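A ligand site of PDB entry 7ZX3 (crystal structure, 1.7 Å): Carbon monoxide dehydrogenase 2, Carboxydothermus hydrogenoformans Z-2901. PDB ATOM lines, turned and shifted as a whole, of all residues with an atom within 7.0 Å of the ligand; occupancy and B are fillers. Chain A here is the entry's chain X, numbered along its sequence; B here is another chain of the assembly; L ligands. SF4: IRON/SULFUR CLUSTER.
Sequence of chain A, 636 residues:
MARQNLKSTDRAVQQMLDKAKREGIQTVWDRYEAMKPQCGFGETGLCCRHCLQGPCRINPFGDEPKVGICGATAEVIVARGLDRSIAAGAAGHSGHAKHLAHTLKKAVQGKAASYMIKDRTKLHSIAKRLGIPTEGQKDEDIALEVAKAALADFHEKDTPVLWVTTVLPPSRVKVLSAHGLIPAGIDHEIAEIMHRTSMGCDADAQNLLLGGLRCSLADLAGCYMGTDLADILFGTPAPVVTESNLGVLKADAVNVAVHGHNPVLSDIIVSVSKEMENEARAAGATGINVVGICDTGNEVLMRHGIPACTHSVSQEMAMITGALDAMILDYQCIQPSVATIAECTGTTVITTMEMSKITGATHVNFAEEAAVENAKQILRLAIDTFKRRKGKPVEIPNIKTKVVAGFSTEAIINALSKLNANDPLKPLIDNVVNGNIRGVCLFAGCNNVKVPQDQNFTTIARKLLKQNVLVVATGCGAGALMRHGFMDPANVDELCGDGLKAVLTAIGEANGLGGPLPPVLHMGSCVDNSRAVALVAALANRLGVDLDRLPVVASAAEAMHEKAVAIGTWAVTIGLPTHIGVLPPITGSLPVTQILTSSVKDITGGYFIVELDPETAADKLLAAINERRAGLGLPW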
ATOM      1  N   CYS A  47     -15.527   8.695  22.798  1.00  0.00           N
ATOM      2  CA  CYS A  47     -16.451   7.717  23.369  1.00  0.00           C
ATOM      3  C   CYS A  47     -16.995   8.301  24.656  1.00  0.00           C
ATOM      4  O   CYS A  47     -16.249   8.946  25.412  1.00  0.00           O
ATOM      5  CB  CYS A  47     -15.803   6.349  23.611  1.00  0.00           C
ATOM      6  SG  CYS A  47     -16.991   5.188  24.383  1.00  0.00           S
ATOM      7  N   CYS A  48     -18.299   8.150  24.864  1.00  0.00           N
ATOM      8  CA  CYS A  48     -18.968   8.649  26.059  1.00  0.00           C
ATOM      9  C   CYS A  48     -19.908   7.581  26.592  1.00  0.00           C
ATOM     10  O   CYS A  48     -20.730   7.047  25.837  1.00  0.00           O
ATOM     11  CB  CYS A  48     -19.773   9.930  25.775  1.00  0.00           C
ATOM     12  SG  CYS A  48     -20.610  10.590  27.209  1.00  0.00           S
ATOM     13  N   ARG A  49     -19.788   7.309  27.900  1.00  0.00           N
ATOM     14  CA  ARG A  49     -20.680   6.425  28.613  1.00  0.00           C
ATOM     15  C   ARG A  49     -21.283   7.136  29.820  1.00  0.00           C
ATOM     16  O   ARG A  49     -21.550   6.494  30.843  1.00  0.00           O
ATOM     17  CB  ARG A  49     -19.964   5.153  29.043  1.00  0.00           C
ATOM     18  CG  ARG A  49     -19.413   4.354  27.866  1.00  0.00           C
ATOM     19  CD  ARG A  49     -18.469   3.251  28.314  1.00  0.00           C
ATOM     20  NE  ARG A  49     -19.099   2.397  29.307  1.00  0.00           N
ATOM     21  CZ  ARG A  49     -18.473   1.669  30.212  1.00  0.00           C
ATOM     22  NH1 ARG A  49     -17.146   1.615  30.281  1.00  0.00           N
ATOM     23  NH2 ARG A  49     -19.203   0.958  31.069  1.00  0.00           N
ATOM     24  N   HIS A  50     -21.526   8.443  29.718  1.00  0.00           N
ATOM     25  CA  HIS A  50     -22.021   9.196  30.878  1.00  0.00           C
ATOM     26  C   HIS A  50     -23.521   9.073  31.066  1.00  0.00           C
ATOM     27  O   HIS A  50     -24.048   9.685  32.007  1.00  0.00           O
ATOM     28  CB  HIS A  50     -21.625  10.683  30.782  1.00  0.00           C
ATOM     29  CG  HIS A  50     -20.151  10.933  30.867  1.00  0.00           C
ATOM     30  ND1 HIS A  50     -19.621  12.186  31.141  1.00  0.00           N
ATOM     31  CD2 HIS A  50     -19.092  10.106  30.702  1.00  0.00           C
ATOM     32  CE1 HIS A  50     -18.300  12.096  31.138  1.00  0.00           C
ATOM     33  NE2 HIS A  50     -17.953  10.853  30.875  1.00  0.00           N
ATOM     34  N   CYS A  51     -24.239   8.322  30.246  1.00  0.00           N
ATOM     35  CA  CYS A  51     -25.607   7.951  30.578  1.00  0.00           C
ATOM     36  C   CYS A  51     -25.950   6.628  29.917  1.00  0.00           C
ATOM     37  O   CYS A  51     -25.167   6.052  29.170  1.00  0.00           O
ATOM     38  CB  CYS A  51     -26.616   9.051  30.190  1.00  0.00           C
ATOM     39  SG  CYS A  51     -27.110   9.068  28.445  1.00  0.00           S
ATOM     40  N   LEU A  52     -27.116   6.100  30.289  1.00  0.00           N
ATOM     41  CA  LEU A  52     -27.528   4.782  29.835  1.00  0.00           C
ATOM     42  C   LEU A  52     -28.146   4.790  28.446  1.00  0.00           C
ATOM     43  O   LEU A  52     -28.589   3.740  27.979  1.00  0.00           O
ATOM     44  CB  LEU A  52     -28.509   4.170  30.850  1.00  0.00           C
ATOM     45  CG  LEU A  52     -27.988   3.936  32.259  1.00  0.00           C
ATOM     46  CD1 LEU A  52     -29.085   3.339  33.144  1.00  0.00           C
ATOM     47  CD2 LEU A  52     -26.772   3.034  32.236  1.00  0.00           C
ATOM     48  N   GLN A  53     -28.185   5.934  27.778  1.00  0.00           N
ATOM     49  CA  GLN A  53     -28.462   5.922  26.349  1.00  0.00           C
ATOM     50  C   GLN A  53     -27.236   5.511  25.544  1.00  0.00           C
ATOM     51  O   GLN A  53     -27.378   5.127  24.369  1.00  0.00           O
ATOM     52  CB  GLN A  53     -28.941   7.298  25.871  1.00  0.00           C
ATOM     53  CG  GLN A  53     -30.310   7.623  26.433  1.00  0.00           C
ATOM     54  CD  GLN A  53     -30.884   8.949  26.019  1.00  0.00           C
ATOM     55  OE1 GLN A  53     -32.101   9.071  25.863  1.00  0.00           O
ATOM     56  NE2 GLN A  53     -30.042   9.975  25.898  1.00  0.00           N
ATOM     57  N   GLY A  54     -26.041   5.605  26.131  1.00  0.00           N
ATOM     58  CA  GLY A  54     -24.827   5.195  25.478  1.00  0.00           C
ATOM     59  C   GLY A  54     -24.654   3.689  25.467  1.00  0.00           C
ATOM     60  O   GLY A  54     -25.535   2.929  25.870  1.00  0.00           O
ATOM     61  N   PRO A  55     -23.474   3.220  25.013  1.00  0.00           N
ATOM     62  CA  PRO A  55     -22.298   4.054  24.722  1.00  0.00           C
ATOM     63  C   PRO A  55     -22.474   4.813  23.432  1.00  0.00           C
ATOM     64  O   PRO A  55     -23.077   4.324  22.465  1.00  0.00           O
ATOM     65  CB  PRO A  55     -21.160   3.047  24.646  1.00  0.00           C
ATOM     66  CG  PRO A  55     -21.773   1.740  24.510  1.00  0.00           C
ATOM     67  CD  PRO A  55     -23.179   1.779  24.941  1.00  0.00           C
ATOM     68  N   CYS A  56     -21.965   6.037  23.441  1.00  0.00           N
ATOM     69  CA  CYS A  56     -21.881   6.855  22.249  1.00  0.00           C
ATOM     70  C   CYS A  56     -20.437   6.955  21.791  1.00  0.00           C
ATOM     71  O   CYS A  56     -19.512   7.021  22.601  1.00  0.00           O
ATOM     72  CB  CYS A  56     -22.438   8.258  22.516  1.00  0.00           C
ATOM     73  SG  CYS A  56     -24.214   8.286  22.759  1.00  0.00           S
ATOM     74  N   ARG A  57     -20.251   6.952  20.483  1.00  0.00           N
ATOM     75  CA  ARG A  57     -18.936   7.115  19.891  1.00  0.00           C
ATOM     76  C   ARG A  57     -19.119   8.057  18.723  1.00  0.00           C
ATOM     77  O   ARG A  57     -20.234   8.279  18.237  1.00  0.00           O
ATOM     78  CB  ARG A  57     -18.323   5.787  19.438  1.00  0.00           C
ATOM     79  CG  ARG A  57     -18.975   5.255  18.180  1.00  0.00           C
ATOM     80  CD  ARG A  57     -18.826   3.781  18.031  1.00  0.00           C
ATOM     81  NE  ARG A  57     -19.454   3.404  16.772  1.00  0.00           N
ATOM     82  CZ  ARG A  57     -20.755   3.180  16.604  1.00  0.00           C
ATOM     83  NH1 ARG A  57     -21.199   2.874  15.388  1.00  0.00           N
ATOM     84  NH2 ARG A  57     -21.626   3.224  17.641  1.00  0.00           N
ATOM     85  N   VAL A  67     -22.046  12.696  16.256  1.00  0.00           N
ATOM     86  CA  VAL A  67     -22.497  13.467  17.393  1.00  0.00           C
ATOM     87  C   VAL A  67     -23.095  12.490  18.392  1.00  0.00           C
ATOM     88  O   VAL A  67     -23.653  11.460  18.005  1.00  0.00           O
ATOM     89  CB  VAL A  67     -23.520  14.558  16.963  1.00  0.00           C
ATOM     90  CG1 VAL A  67     -24.809  13.927  16.388  1.00  0.00           C
ATOM     91  CG2 VAL A  67     -23.834  15.496  18.095  1.00  0.00           C
ATOM     92  N   GLY A  68     -22.971  12.792  19.676  1.00  0.00           N
ATOM     93  CA  GLY A  68     -23.609  11.955  20.683  1.00  0.00           C
ATOM     94  C   GLY A  68     -25.127  12.000  20.603  1.00  0.00           C
ATOM     95  O   GLY A  68     -25.718  12.892  20.022  1.00  0.00           O
ATOM     96  N   ILE A  69     -25.763  11.009  21.211  1.00  0.00           N
ATOM     97  CA  ILE A  69     -27.212  10.878  21.090  1.00  0.00           C
ATOM     98  C   ILE A  69     -27.916  12.101  21.664  1.00  0.00           C
ATOM     99  O   ILE A  69     -28.917  12.581  21.104  1.00  0.00           O
ATOM    100  CB  ILE A  69     -27.679   9.574  21.752  1.00  0.00           C
ATOM    101  CG1 ILE A  69     -27.292   8.386  20.892  1.00  0.00           C
ATOM    102  CG2 ILE A  69     -29.194   9.651  22.076  1.00  0.00           C
ATOM    103  CD1 ILE A  69     -27.462   7.020  21.551  1.00  0.00           C
ATOM    104  N   CYS A  70     -27.408  12.644  22.783  1.00  0.00           N
ATOM    105  CA  CYS A  70     -28.001  13.810  23.406  1.00  0.00           C
ATOM    106  C   CYS A  70     -27.611  15.100  22.703  1.00  0.00           C
ATOM    107  O   CYS A  70     -28.100  16.175  23.102  1.00  0.00           O
ATOM    108  CB  CYS A  70     -27.567  13.899  24.861  1.00  0.00           C
ATOM    109  SG  CYS A  70     -25.772  14.059  25.008  1.00  0.00           S
ATOM    110  N   GLY A  71     -26.783  15.006  21.662  1.00  0.00           N
ATOM    111  CA  GLY A  71     -26.277  16.182  20.984  1.00  0.00           C
ATOM    112  C   GLY A  71     -24.895  16.613  21.414  1.00  0.00           C
ATOM    113  O   GLY A  71     -24.418  17.661  20.944  1.00  0.00           O
ATOM    114  N   ALA A  72     -24.233  15.847  22.273  1.00  0.00           N
ATOM    115  CA  ALA A  72     -22.882  16.178  22.728  1.00  0.00           C
ATOM    116  C   ALA A  72     -21.915  16.073  21.555  1.00  0.00           C
ATOM    117  O   ALA A  72     -21.822  15.032  20.905  1.00  0.00           O
ATOM    118  CB  ALA A  72     -22.449  15.236  23.842  1.00  0.00           C
ATOM    119  N   THR A  73     -21.230  17.169  21.258  1.00  0.00           N
ATOM    120  CA  THR A  73     -20.278  17.198  20.167  1.00  0.00           C
ATOM    121  C   THR A  73     -18.978  16.499  20.550  1.00  0.00           C
ATOM    122  O   THR A  73     -18.712  16.211  21.705  1.00  0.00           O
ATOM    123  CB  THR A  73     -19.931  18.629  19.788  1.00  0.00           C
ATOM    124  OG1 THR A  73     -19.374  19.263  20.935  1.00  0.00           O
ATOM    125  CG2 THR A  73     -21.156  19.409  19.298  1.00  0.00           C
ATOM    126  N   ILE A  77     -17.527  15.900  24.312  1.00  0.00           N
ATOM    127  CA  ILE A  77     -17.203  14.555  24.803  1.00  0.00           C
ATOM    128  C   ILE A  77     -15.746  14.475  25.243  1.00  0.00           C
ATOM    129  O   ILE A  77     -15.426  13.914  26.309  1.00  0.00           O
ATOM    130  CB  ILE A  77     -17.537  13.502  23.730  1.00  0.00           C
ATOM    131  CG1 ILE A  77     -19.064  13.376  23.626  1.00  0.00           C
ATOM    132  CG2 ILE A  77     -16.876  12.136  24.029  1.00  0.00           C
ATOM    133  CD1 ILE A  77     -19.581  12.627  22.457  1.00  0.00           C
ATOM    134  N   ARG A  80     -15.146  16.524  28.444  1.00  0.00           N
ATOM    135  CA  ARG A  80     -15.764  15.946  29.644  1.00  0.00           C
ATOM    136  C   ARG A  80     -14.971  14.750  30.134  1.00  0.00           C
ATOM    137  O   ARG A  80     -14.804  14.547  31.342  1.00  0.00           O
ATOM    138  CB  ARG A  80     -17.212  15.542  29.349  1.00  0.00           C
ATOM    139  CG  ARG A  80     -18.144  16.721  29.230  1.00  0.00           C
ATOM    140  CD  ARG A  80     -19.628  16.324  29.188  1.00  0.00           C
ATOM    141  NE  ARG A  80     -19.903  15.232  28.257  1.00  0.00           N
ATOM    142  CZ  ARG A  80     -21.134  14.936  27.853  1.00  0.00           C
ATOM    143  NH1 ARG A  80     -22.162  15.610  28.312  1.00  0.00           N
ATOM    144  NH2 ARG A  80     -21.339  13.929  27.011  1.00  0.00           N
ATOM    145  N   THR A 197     -19.880  17.466  34.150  1.00  0.00           N
ATOM    146  CA  THR A 197     -19.616  16.550  33.062  1.00  0.00           C
ATOM    147  C   THR A 197     -20.678  15.463  32.935  1.00  0.00           C
ATOM    148  O   THR A 197     -20.594  14.662  31.985  1.00  0.00           O
ATOM    149  CB  THR A 197     -18.246  15.876  33.232  1.00  0.00           C
ATOM    150  OG1 THR A 197     -18.210  15.135  34.462  1.00  0.00           O
ATOM    151  CG2 THR A 197     -17.075  16.907  33.207  1.00  0.00           C
ATOM    152  N   SER A 198     -21.640  15.412  33.852  1.00  0.00           N
ATOM    153  CA  SER A 198     -22.722  14.446  33.745  1.00  0.00           C
ATOM    154  C   SER A 198     -23.679  14.881  32.627  1.00  0.00           C
ATOM    155  O   SER A 198     -23.552  15.964  32.058  1.00  0.00           O
ATOM    156  CB  SER A 198     -23.450  14.276  35.091  1.00  0.00           C
ATOM    157  OG  SER A 198     -24.268  15.380  35.396  1.00  0.00           O
ATOM    158  N   MET A 199     -24.576  13.970  32.254  1.00  0.00           N
ATOM    159  CA  MET A 199     -25.350  14.212  31.047  1.00  0.00           C
ATOM    160  C   MET A 199     -26.204  15.459  31.205  1.00  0.00           C
ATOM    161  O   MET A 199     -26.796  15.721  32.276  1.00  0.00           O
ATOM    162  CB  MET A 199     -26.231  13.003  30.716  1.00  0.00           C
ATOM    163  CG  MET A 199     -27.127  13.149  29.496  1.00  0.00           C
ATOM    164  SD  MET A 199     -28.660  13.980  29.884  1.00  0.00           S
ATOM    165  CE  MET A 199     -29.531  13.770  28.342  1.00  0.00           C
ATOM    166  N   GLY A 200     -26.265  16.241  30.136  1.00  0.00           N
ATOM    167  CA  GLY A 200     -27.157  17.381  30.090  1.00  0.00           C
ATOM    168  C   GLY A 200     -26.714  18.582  30.898  1.00  0.00           C
ATOM    169  O   GLY A 200     -27.554  19.379  31.297  1.00  0.00           O
ATOM    170  N   VAL B  28     -33.123  13.648  18.693  1.00  0.00           N
ATOM    171  CA  VAL B  28     -32.479  12.629  19.518  1.00  0.00           C
ATOM    172  C   VAL B  28     -32.662  11.230  18.918  1.00  0.00           C
ATOM    173  O   VAL B  28     -31.758  10.403  18.973  1.00  0.00           O
ATOM    174  CB  VAL B  28     -33.021  12.711  20.960  1.00  0.00           C
ATOM    175  CG1 VAL B  28     -34.514  12.388  21.025  1.00  0.00           C
ATOM    176  CG2 VAL B  28     -32.194  11.809  21.905  1.00  0.00           C
ATOM    177  N   MET B  35     -26.298   5.969  15.693  1.00  0.00           N
ATOM    178  CA  MET B  35     -25.330   5.375  16.593  1.00  0.00           C
ATOM    179  C   MET B  35     -25.384   3.858  16.607  1.00  0.00           C
ATOM    180  O   MET B  35     -24.500   3.211  17.185  1.00  0.00           O
ATOM    181  CB  MET B  35     -25.567   5.928  18.009  1.00  0.00           C
ATOM    182  CG  MET B  35     -24.467   5.691  18.984  1.00  0.00           C
ATOM    183  SD  MET B  35     -22.954   6.575  18.564  1.00  0.00           S
ATOM    184  CE  MET B  35     -23.419   8.270  18.771  1.00  0.00           C
ATOM    185  N   GLN B  38     -24.680  -0.045  18.780  1.00  0.00           N
ATOM    186  CA  GLN B  38     -23.837   0.511  19.816  1.00  0.00           C
ATOM    187  C   GLN B  38     -22.815  -0.509  20.309  1.00  0.00           C
ATOM    188  O   GLN B  38     -22.989  -1.733  20.224  1.00  0.00           O
ATOM    189  CB  GLN B  38     -24.697   1.004  20.977  1.00  0.00           C
ATOM    190  CG  GLN B  38     -25.614   2.127  20.564  1.00  0.00           C
ATOM    191  CD  GLN B  38     -26.465   2.663  21.674  1.00  0.00           C
ATOM    192  OE1 GLN B  38     -27.569   2.185  21.888  1.00  0.00           O
ATOM    193  NE2 GLN B  38     -25.965   3.687  22.357  1.00  0.00           N
ATOM    194  N   PRO B 336     -27.829  19.084  24.749  1.00  0.00           N
ATOM    195  CA  PRO B 336     -27.170  20.267  24.199  1.00  0.00           C
ATOM    196  C   PRO B 336     -27.548  20.546  22.765  1.00  0.00           C
ATOM    197  O   PRO B 336     -27.303  21.661  22.297  1.00  0.00           O
ATOM    198  CB  PRO B 336     -25.679  19.946  24.330  1.00  0.00           C
ATOM    199  CG  PRO B 336     -25.590  18.480  24.527  1.00  0.00           C
ATOM    200  CD  PRO B 336     -26.848  18.104  25.251  1.00  0.00           C
ATOM    201  N   MET B 560     -31.982   6.675  32.546  1.00  0.00           N
ATOM    202  CA  MET B 560     -30.977   7.245  31.651  1.00  0.00           C
ATOM    203  C   MET B 560     -29.793   7.866  32.395  1.00  0.00           C
ATOM    204  O   MET B 560     -28.639   7.494  32.164  1.00  0.00           O
ATOM    205  CB  MET B 560     -31.634   8.313  30.772  1.00  0.00           C
ATOM    206  CG  MET B 560     -30.723   8.990  29.775  1.00  0.00           C
ATOM    207  SD  MET B 560     -29.993  10.536  30.389  1.00  0.00           S
ATOM    208  CE  MET B 560     -31.405  11.585  30.681  1.00  0.00           C
HETATM  209 FE1  SF4 L   1     -24.391   9.531  24.726  1.00  0.00          FE
HETATM  210 FE2  SF4 L   1     -22.822  10.541  26.611  1.00  0.00          FE
HETATM  211 FE3  SF4 L   1     -25.335   9.833  27.222  1.00  0.00          FE
HETATM  212 FE4  SF4 L   1     -24.862  12.042  25.640  1.00  0.00          FE
HETATM  213  S1  SF4 L   1     -24.224  11.771  27.860  1.00  0.00           S
HETATM  214  S2  SF4 L   1     -26.365  10.357  25.215  1.00  0.00           S
HETATM  215  S3  SF4 L   1     -23.058  11.371  24.513  1.00  0.00           S
HETATM  216  S4  SF4 L   1     -23.672   8.459  26.617  1.00  0.00           S
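An iron atom (FE4) of the ligand is bound by the side-chain sulfur (SG) of Cys 70. FE2 of the ligand is bound by SG of Cys 48 (2.3 Å). SG of Cys 56 is bound to FE1 of the ligand (2.3 Å). A sulfur (S4) of the ligand lies close to the backbone NH (N) of Cys 51 (3.7 Å). S2 of the ligand lies close to NE2 of Gln 53 (3.8 Å). A sulfur (S1) of the ligand sits close to the guanidinium group (NH2) of Arg 80, 3.7 Å away. N of Cys 70 lies close to S2 of the ligand (3.5 Å). N of Gly 54 sits close to S4 of the ligand, 3.7 Å away. N of His 50 sits close to S4 of the ligand (3.8 Å). An iron atom (FE3) of the ligand is bound by the side-chain sulfur (SG) of Cys 51.
SG of Cys 51 lies close to N of Gln 53, 3.4 Å away. NE2 of Gln 38 of chain B sits at hydrogen-bond distance from O of Gln 53 (2.8 Å). The backbone carbonyl oxygen of Cys 56 lies close to the side-chain sulfur of Cys 47, at 3.6 Å. The side-chain sulfur of Cys 70 lies close to the backbone NH of Ala 72 (3.6 Å). A ring nitrogen (ND1) of His 50 is in hydrogen-bond range of the backbone carbonyl oxygen (O) of Thr 197 (2.8 Å). O of Cys 56 lies within hydrogen-bond range of N of Cys 48. The side-chain sulfur (SG) of Cys 56 lies close to the backbone NH (N) of Ile 69, 3.5 Å away. The side-chain sulfur (SD) of Met 560 of chain B lies close to the side-chain sulfur (SG) of Cys 51 (3.8 Å).
CA of Gly 68 touches S3 of the ligand (3.9 Å). Ile 69 touches the ligand (CB to S2, 3.8 Å). Ala 72 touches the ligand (CB to S3, 3.97 Å). Met 199 touches the ligand (CG to S1, 3.6 Å).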
